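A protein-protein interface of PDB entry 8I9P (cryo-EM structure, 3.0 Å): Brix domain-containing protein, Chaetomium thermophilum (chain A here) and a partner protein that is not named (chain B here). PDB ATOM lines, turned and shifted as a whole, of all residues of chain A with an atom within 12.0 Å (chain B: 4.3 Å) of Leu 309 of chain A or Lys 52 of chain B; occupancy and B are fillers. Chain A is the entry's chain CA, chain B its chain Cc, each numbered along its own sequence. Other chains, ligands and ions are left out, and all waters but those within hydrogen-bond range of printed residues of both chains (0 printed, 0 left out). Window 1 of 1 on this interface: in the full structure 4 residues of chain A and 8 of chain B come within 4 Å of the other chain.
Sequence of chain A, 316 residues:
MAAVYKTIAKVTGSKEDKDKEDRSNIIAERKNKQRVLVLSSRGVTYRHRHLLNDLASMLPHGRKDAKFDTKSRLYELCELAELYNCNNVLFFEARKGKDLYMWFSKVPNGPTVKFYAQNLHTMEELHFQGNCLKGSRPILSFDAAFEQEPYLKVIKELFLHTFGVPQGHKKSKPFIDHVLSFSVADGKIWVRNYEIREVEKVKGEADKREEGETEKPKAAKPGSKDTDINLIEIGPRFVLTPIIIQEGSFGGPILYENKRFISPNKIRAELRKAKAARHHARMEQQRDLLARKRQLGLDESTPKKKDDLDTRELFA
Among the printed residues, merely in contact across the chains: Phe 315 of chain A with Tyr 56 of chain B (3.5 Å), Leu 309 of chain A with Arg 99 of chain B (3.7 Å), Leu 309 of chain A with Lys 49 of chain B (3.7 Å), Leu 314 of chain A with Lys 49 of chain B (3.8 Å), Leu 309 of chain A with Leu 48 of chain B (3.8 Å) and Leu 309 of chain A with Lys 52 of chain B (3.8 Å).
NZ of Lys 52 of chain B lies within hydrogen-bond range of OG1 of Thr 311 of chain A (3.4 Å).
Lys 52 of chain B touches just these residues of chain A: Leu 309 (3.8 Å) and Thr 311 (3.4 Å). Printed residues of chain A within 4 Å of Lys 49 of chain B: Leu 309 and Leu 314. Gly 53 of chain B touches none of the printed residues of chain A. No residue of chain A comes within 4 Å of Phe 55 of chain B. Of chain A, only Phe 315 (3.5 Å) comes within 4 Å of Tyr 56 of chain B. No residue of chain A comes within 4 Å of Thr 96 of chain B. Printed residues of chain B within 4 Å of Thr 311 of chain A: Lys 52. Of the printed residues of chain B, Leu 314 of chain A touches Lys 49. Printed residues of chain A within 4 Å of Arg 99 of chain B: Leu 309 (3.7 Å). Of the printed residues of chain B, Phe 315 of chain A touches Tyr 56 (3.5 Å). The nearest residue of chain B that does not touch Leu 309 of chain A is Ile 185 of chain B (4.2 Å). The nearest printed residue of chain B that does not touch Leu 314 of chain A is Lys 52 of chain B (4.3 Å).
Hydrophobic or aromatic side chains of chain A within 4 Å of the printed part of chain B: Leu 309, Leu 314 and Phe 315. Hydrophobic or aromatic side chains of chain B that line the printed part of chain A: Leu 48 and Tyr 56. Among the printed residues, 7 pairs touch across the chains.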
ATOM      1  N   ASP A 308      -1.202  -7.235 -22.648  1.00  0.00           N
ATOM      2  CA  ASP A 308      -1.023  -5.788 -22.687  1.00  0.00           C
ATOM      3  C   ASP A 308      -2.324  -5.077 -22.343  1.00  0.00           C
ATOM      4  O   ASP A 308      -2.319  -4.004 -21.741  1.00  0.00           O
ATOM      5  CB  ASP A 308      -0.523  -5.344 -24.060  1.00  0.00           C
ATOM      6  CG  ASP A 308       0.618  -4.355 -23.968  1.00  0.00           C
ATOM      7  OD1 ASP A 308       0.721  -3.663 -22.933  1.00  0.00           O
ATOM      8  OD2 ASP A 308       1.416  -4.272 -24.925  1.00  0.00           O
ATOM      9  N   LEU A 309      -3.444  -5.687 -22.734  1.00  0.00           N
ATOM     10  CA  LEU A 309      -4.769  -5.202 -22.354  1.00  0.00           C
ATOM     11  C   LEU A 309      -5.150  -5.766 -20.983  1.00  0.00           C
ATOM     12  O   LEU A 309      -6.069  -6.569 -20.824  1.00  0.00           O
ATOM     13  CB  LEU A 309      -5.790  -5.571 -23.422  1.00  0.00           C
ATOM     14  CG  LEU A 309      -7.150  -4.873 -23.374  1.00  0.00           C
ATOM     15  CD1 LEU A 309      -6.980  -3.368 -23.397  1.00  0.00           C
ATOM     16  CD2 LEU A 309      -8.016  -5.337 -24.529  1.00  0.00           C
ATOM     17  N   ASP A 310      -4.395  -5.335 -19.979  1.00  0.00           N
ATOM     18  CA  ASP A 310      -4.557  -5.798 -18.611  1.00  0.00           C
ATOM     19  C   ASP A 310      -4.449  -4.607 -17.674  1.00  0.00           C
ATOM     20  O   ASP A 310      -3.804  -3.610 -18.004  1.00  0.00           O
ATOM     21  CB  ASP A 310      -3.509  -6.857 -18.254  1.00  0.00           C
ATOM     22  CG  ASP A 310      -3.868  -7.632 -17.005  1.00  0.00           C
ATOM     23  OD1 ASP A 310      -5.032  -7.539 -16.564  1.00  0.00           O
ATOM     24  OD2 ASP A 310      -2.987  -8.332 -16.465  1.00  0.00           O
ATOM     25  N   THR A 311      -5.094  -4.717 -16.510  1.00  0.00           N
ATOM     26  CA  THR A 311      -5.123  -3.612 -15.556  1.00  0.00           C
ATOM     27  C   THR A 311      -3.729  -3.302 -15.019  1.00  0.00           C
ATOM     28  O   THR A 311      -3.325  -2.135 -14.938  1.00  0.00           O
ATOM     29  CB  THR A 311      -6.092  -3.950 -14.420  1.00  0.00           C
ATOM     30  OG1 THR A 311      -7.440  -3.767 -14.874  1.00  0.00           O
ATOM     31  CG2 THR A 311      -5.849  -3.082 -13.193  1.00  0.00           C
ATOM     32  N   ARG A 312      -2.957  -4.335 -14.704  1.00  0.00           N
ATOM     33  CA  ARG A 312      -1.666  -4.154 -14.042  1.00  0.00           C
ATOM     34  C   ARG A 312      -0.523  -4.015 -15.045  1.00  0.00           C
ATOM     35  O   ARG A 312       0.653  -4.104 -14.697  1.00  0.00           O
ATOM     36  CB  ARG A 312      -1.424  -5.314 -13.089  1.00  0.00           C
ATOM     37  CG  ARG A 312      -1.792  -6.658 -13.666  1.00  0.00           C
ATOM     38  CD  ARG A 312      -2.409  -7.571 -12.615  1.00  0.00           C
ATOM     39  NE  ARG A 312      -3.576  -6.977 -11.967  1.00  0.00           N
ATOM     40  CZ  ARG A 312      -3.623  -6.554 -10.710  1.00  0.00           C
ATOM     41  NH1 ARG A 312      -2.575  -6.646  -9.908  1.00  0.00           N
ATOM     42  NH2 ARG A 312      -4.756  -6.038 -10.242  1.00  0.00           N
ATOM     43  N   GLU A 313      -0.872  -3.782 -16.309  1.00  0.00           N
ATOM     44  CA  GLU A 313       0.114  -3.600 -17.366  1.00  0.00           C
ATOM     45  C   GLU A 313      -0.149  -2.292 -18.100  1.00  0.00           C
ATOM     46  O   GLU A 313       0.747  -1.736 -18.742  1.00  0.00           O
ATOM     47  CB  GLU A 313       0.079  -4.773 -18.345  1.00  0.00           C
ATOM     48  CG  GLU A 313       0.627  -6.073 -17.790  1.00  0.00           C
ATOM     49  CD  GLU A 313       2.120  -6.217 -18.007  1.00  0.00           C
ATOM     50  OE1 GLU A 313       2.611  -5.799 -19.077  1.00  0.00           O
ATOM     51  OE2 GLU A 313       2.801  -6.754 -17.108  1.00  0.00           O
ATOM     52  N   LEU A 314      -1.382  -1.800 -18.006  1.00  0.00           N
ATOM     53  CA  LEU A 314      -1.793  -0.550 -18.627  1.00  0.00           C
ATOM     54  C   LEU A 314      -1.868   0.612 -17.653  1.00  0.00           C
ATOM     55  O   LEU A 314      -1.544   1.739 -18.029  1.00  0.00           O
ATOM     56  CB  LEU A 314      -3.162  -0.722 -19.298  1.00  0.00           C
ATOM     57  CG  LEU A 314      -3.723   0.416 -20.145  1.00  0.00           C
ATOM     58  CD1 LEU A 314      -2.781   0.763 -21.283  1.00  0.00           C
ATOM     59  CD2 LEU A 314      -5.102   0.056 -20.667  1.00  0.00           C
ATOM     60  N   PHE A 315      -2.278   0.361 -16.411  1.00  0.00           N
ATOM     61  CA  PHE A 315      -2.391   1.399 -15.396  1.00  0.00           C
ATOM     62  C   PHE A 315      -1.203   1.414 -14.446  1.00  0.00           C
ATOM     63  O   PHE A 315      -1.257   2.091 -13.415  1.00  0.00           O
ATOM     64  CB  PHE A 315      -3.696   1.229 -14.616  1.00  0.00           C
ATOM     65  CG  PHE A 315      -4.922   1.490 -15.437  1.00  0.00           C
ATOM     66  CD1 PHE A 315      -5.383   2.781 -15.621  1.00  0.00           C
ATOM     67  CD2 PHE A 315      -5.606   0.448 -16.036  1.00  0.00           C
ATOM     68  CE1 PHE A 315      -6.504   3.028 -16.384  1.00  0.00           C
ATOM     69  CE2 PHE A 315      -6.730   0.689 -16.797  1.00  0.00           C
ATOM     70  CZ  PHE A 315      -7.177   1.982 -16.972  1.00  0.00           C
ATOM     71  N   ALA A 316      -0.138   0.688 -14.764  1.00  0.00           N
ATOM     72  CA  ALA A 316       1.056   0.671 -13.931  1.00  0.00           C
ATOM     73  C   ALA A 316       1.821   1.985 -14.058  1.00  0.00           C
ATOM     74  O   ALA A 316       3.051   2.000 -14.065  1.00  0.00           O
ATOM     75  CB  ALA A 316       1.947  -0.500 -14.305  1.00  0.00           C
ATOM     76  N   LEU B  48      -8.615  -0.342 -28.132  1.00  0.00           N
ATOM     77  CA  LEU B  48      -9.061  -1.083 -26.954  1.00  0.00           C
ATOM     78  C   LEU B  48      -8.495  -0.527 -25.652  1.00  0.00           C
ATOM     79  O   LEU B  48      -9.250  -0.359 -24.688  1.00  0.00           O
ATOM     80  CB  LEU B  48      -8.693  -2.563 -27.077  1.00  0.00           C
ATOM     81  CG  LEU B  48      -9.569  -3.415 -27.996  1.00  0.00           C
ATOM     82  CD1 LEU B  48      -8.975  -4.801 -28.163  1.00  0.00           C
ATOM     83  CD2 LEU B  48     -10.984  -3.496 -27.460  1.00  0.00           C
ATOM     84  N   LYS B  49      -7.198  -0.221 -25.605  1.00  0.00           N
ATOM     85  CA  LYS B  49      -6.596   0.397 -24.429  1.00  0.00           C
ATOM     86  C   LYS B  49      -7.140   1.793 -24.144  1.00  0.00           C
ATOM     87  O   LYS B  49      -7.431   2.108 -22.979  1.00  0.00           O
ATOM     88  CB  LYS B  49      -5.074   0.455 -24.590  1.00  0.00           C
ATOM     89  CG  LYS B  49      -4.383  -0.863 -24.278  1.00  0.00           C
ATOM     90  CD  LYS B  49      -3.199  -1.134 -25.189  1.00  0.00           C
ATOM     91  CE  LYS B  49      -2.252   0.046 -25.248  1.00  0.00           C
ATOM     92  NZ  LYS B  49      -0.834  -0.400 -25.308  1.00  0.00           N
ATOM     93  N   LEU B  50      -7.309   2.620 -25.177  1.00  0.00           N
ATOM     94  CA  LEU B  50      -7.922   3.934 -25.028  1.00  0.00           C
ATOM     95  C   LEU B  50      -9.351   3.843 -24.514  1.00  0.00           C
ATOM     96  O   LEU B  50      -9.747   4.634 -23.654  1.00  0.00           O
ATOM     97  CB  LEU B  50      -7.905   4.687 -26.362  1.00  0.00           C
ATOM     98  CG  LEU B  50      -6.562   5.161 -26.921  1.00  0.00           C
ATOM     99  CD1 LEU B  50      -6.643   5.289 -28.430  1.00  0.00           C
ATOM    100  CD2 LEU B  50      -6.158   6.482 -26.306  1.00  0.00           C
ATOM    101  N   TRP B  51     -10.132   2.878 -25.003  1.00  0.00           N
ATOM    102  CA  TRP B  51     -11.504   2.758 -24.534  1.00  0.00           C
ATOM    103  C   TRP B  51     -11.577   2.164 -23.136  1.00  0.00           C
ATOM    104  O   TRP B  51     -12.528   2.448 -22.406  1.00  0.00           O
ATOM    105  CB  TRP B  51     -12.331   1.935 -25.518  1.00  0.00           C
ATOM    106  CG  TRP B  51     -13.003   2.788 -26.546  1.00  0.00           C
ATOM    107  CD1 TRP B  51     -12.780   2.776 -27.889  1.00  0.00           C
ATOM    108  CD2 TRP B  51     -13.993   3.798 -26.314  1.00  0.00           C
ATOM    109  NE1 TRP B  51     -13.574   3.706 -28.510  1.00  0.00           N
ATOM    110  CE2 TRP B  51     -14.327   4.349 -27.564  1.00  0.00           C
ATOM    111  CE3 TRP B  51     -14.635   4.285 -25.170  1.00  0.00           C
ATOM    112  CZ2 TRP B  51     -15.275   5.358 -27.705  1.00  0.00           C
ATOM    113  CZ3 TRP B  51     -15.570   5.290 -25.313  1.00  0.00           C
ATOM    114  CH2 TRP B  51     -15.881   5.816 -26.570  1.00  0.00           C
ATOM    115  N   LYS B  52     -10.592   1.355 -22.737  1.00  0.00           N
ATOM    116  CA  LYS B  52     -10.505   0.951 -21.335  1.00  0.00           C
ATOM    117  C   LYS B  52     -10.251   2.155 -20.435  1.00  0.00           C
ATOM    118  O   LYS B  52     -10.871   2.295 -19.367  1.00  0.00           O
ATOM    119  CB  LYS B  52      -9.403  -0.093 -21.159  1.00  0.00           C
ATOM    120  CG  LYS B  52      -9.640  -1.064 -20.019  1.00  0.00           C
ATOM    121  CD  LYS B  52      -8.842  -2.339 -20.212  1.00  0.00           C
ATOM    122  CE  LYS B  52      -8.034  -2.677 -18.975  1.00  0.00           C
ATOM    123  NZ  LYS B  52      -8.842  -3.406 -17.963  1.00  0.00           N
ATOM    124  N   GLY B  53      -9.352   3.044 -20.867  1.00  0.00           N
ATOM    125  CA  GLY B  53      -9.124   4.277 -20.126  1.00  0.00           C
ATOM    126  C   GLY B  53     -10.359   5.157 -20.046  1.00  0.00           C
ATOM    127  O   GLY B  53     -10.663   5.720 -18.992  1.00  0.00           O
ATOM    128  N   LEU B  54     -11.098   5.271 -21.153  1.00  0.00           N
ATOM    129  CA  LEU B  54     -12.333   6.053 -21.144  1.00  0.00           C
ATOM    130  C   LEU B  54     -13.419   5.397 -20.300  1.00  0.00           C
ATOM    131  O   LEU B  54     -14.222   6.098 -19.669  1.00  0.00           O
ATOM    132  CB  LEU B  54     -12.838   6.268 -22.570  1.00  0.00           C
ATOM    133  CG  LEU B  54     -11.901   7.040 -23.494  1.00  0.00           C
ATOM    134  CD1 LEU B  54     -12.515   7.241 -24.866  1.00  0.00           C
ATOM    135  CD2 LEU B  54     -11.549   8.360 -22.863  1.00  0.00           C
ATOM    136  N   PHE B  55     -13.460   4.061 -20.283  1.00  0.00           N
ATOM    137  CA  PHE B  55     -14.387   3.339 -19.422  1.00  0.00           C
ATOM    138  C   PHE B  55     -14.139   3.672 -17.963  1.00  0.00           C
ATOM    139  O   PHE B  55     -15.077   3.981 -17.223  1.00  0.00           O
ATOM    140  CB  PHE B  55     -14.255   1.832 -19.658  1.00  0.00           C
ATOM    141  CG  PHE B  55     -15.086   0.988 -18.727  1.00  0.00           C
ATOM    142  CD1 PHE B  55     -16.417   0.739 -19.007  1.00  0.00           C
ATOM    143  CD2 PHE B  55     -14.532   0.423 -17.586  1.00  0.00           C
ATOM    144  CE1 PHE B  55     -17.185  -0.032 -18.160  1.00  0.00           C
ATOM    145  CE2 PHE B  55     -15.296  -0.346 -16.736  1.00  0.00           C
ATOM    146  CZ  PHE B  55     -16.623  -0.576 -17.025  1.00  0.00           C
ATOM    147  N   TYR B  56     -12.878   3.642 -17.533  1.00  0.00           N
ATOM    148  CA  TYR B  56     -12.599   4.001 -16.147  1.00  0.00           C
ATOM    149  C   TYR B  56     -12.767   5.492 -15.873  1.00  0.00           C
ATOM    150  O   TYR B  56     -13.125   5.862 -14.745  1.00  0.00           O
ATOM    151  CB  TYR B  56     -11.204   3.524 -15.751  1.00  0.00           C
ATOM    152  CG  TYR B  56     -11.184   2.043 -15.473  1.00  0.00           C
ATOM    153  CD1 TYR B  56     -11.874   1.519 -14.389  1.00  0.00           C
ATOM    154  CD2 TYR B  56     -10.507   1.166 -16.306  1.00  0.00           C
ATOM    155  CE1 TYR B  56     -11.876   0.166 -14.132  1.00  0.00           C
ATOM    156  CE2 TYR B  56     -10.500  -0.190 -16.057  1.00  0.00           C
ATOM    157  CZ  TYR B  56     -11.187  -0.685 -14.968  1.00  0.00           C
ATOM    158  OH  TYR B  56     -11.184  -2.034 -14.716  1.00  0.00           O
ATOM    159  N   THR B  96     -15.285  -3.029 -25.773  1.00  0.00           N
ATOM    160  CA  THR B  96     -15.161  -2.693 -24.357  1.00  0.00           C
ATOM    161  C   THR B  96     -16.497  -2.836 -23.637  1.00  0.00           C
ATOM    162  O   THR B  96     -16.562  -3.397 -22.534  1.00  0.00           O
ATOM    163  CB  THR B  96     -14.616  -1.273 -24.206  1.00  0.00           C
ATOM    164  OG1 THR B  96     -13.314  -1.197 -24.800  1.00  0.00           O
ATOM    165  CG2 THR B  96     -14.514  -0.885 -22.741  1.00  0.00           C
ATOM    166  N   ARG B  99     -17.223  -6.519 -23.230  1.00  0.00           N
ATOM    167  CA  ARG B  99     -16.401  -7.089 -22.172  1.00  0.00           C
ATOM    168  C   ARG B  99     -16.901  -6.732 -20.783  1.00  0.00           C
ATOM    169  O   ARG B  99     -16.957  -7.606 -19.910  1.00  0.00           O
ATOM    170  CB  ARG B  99     -14.950  -6.618 -22.306  1.00  0.00           C
ATOM    171  CG  ARG B  99     -14.005  -7.258 -21.301  1.00  0.00           C
ATOM    172  CD  ARG B  99     -12.552  -6.929 -21.591  1.00  0.00           C
ATOM    173  NE  ARG B  99     -12.284  -5.501 -21.490  1.00  0.00           N
ATOM    174  CZ  ARG B  99     -11.847  -4.748 -22.490  1.00  0.00           C
ATOM    175  NH1 ARG B  99     -11.615  -5.257 -23.687  1.00  0.00           N
ATOM    176  NH2 ARG B  99     -11.636  -3.452 -22.282  1.00  0.00           N
ATOM    177  N   ILE B 185      -8.781 -12.278 -29.624  1.00  0.00           N
ATOM    178  CA  ILE B 185      -9.719 -11.882 -28.578  1.00  0.00           C
ATOM    179  C   ILE B 185     -11.093 -12.387 -28.994  1.00  0.00           C
ATOM    180  O   ILE B 185     -11.690 -11.885 -29.951  1.00  0.00           O
ATOM    181  CB  ILE B 185      -9.726 -10.369 -28.342  1.00  0.00           C
ATOM    182  CG1 ILE B 185      -8.330  -9.893 -27.916  1.00  0.00           C
ATOM    183  CG2 ILE B 185     -10.802 -10.003 -27.324  1.00  0.00           C
ATOM    184  CD1 ILE B 185      -8.308  -8.601 -27.120  1.00  0.00           C
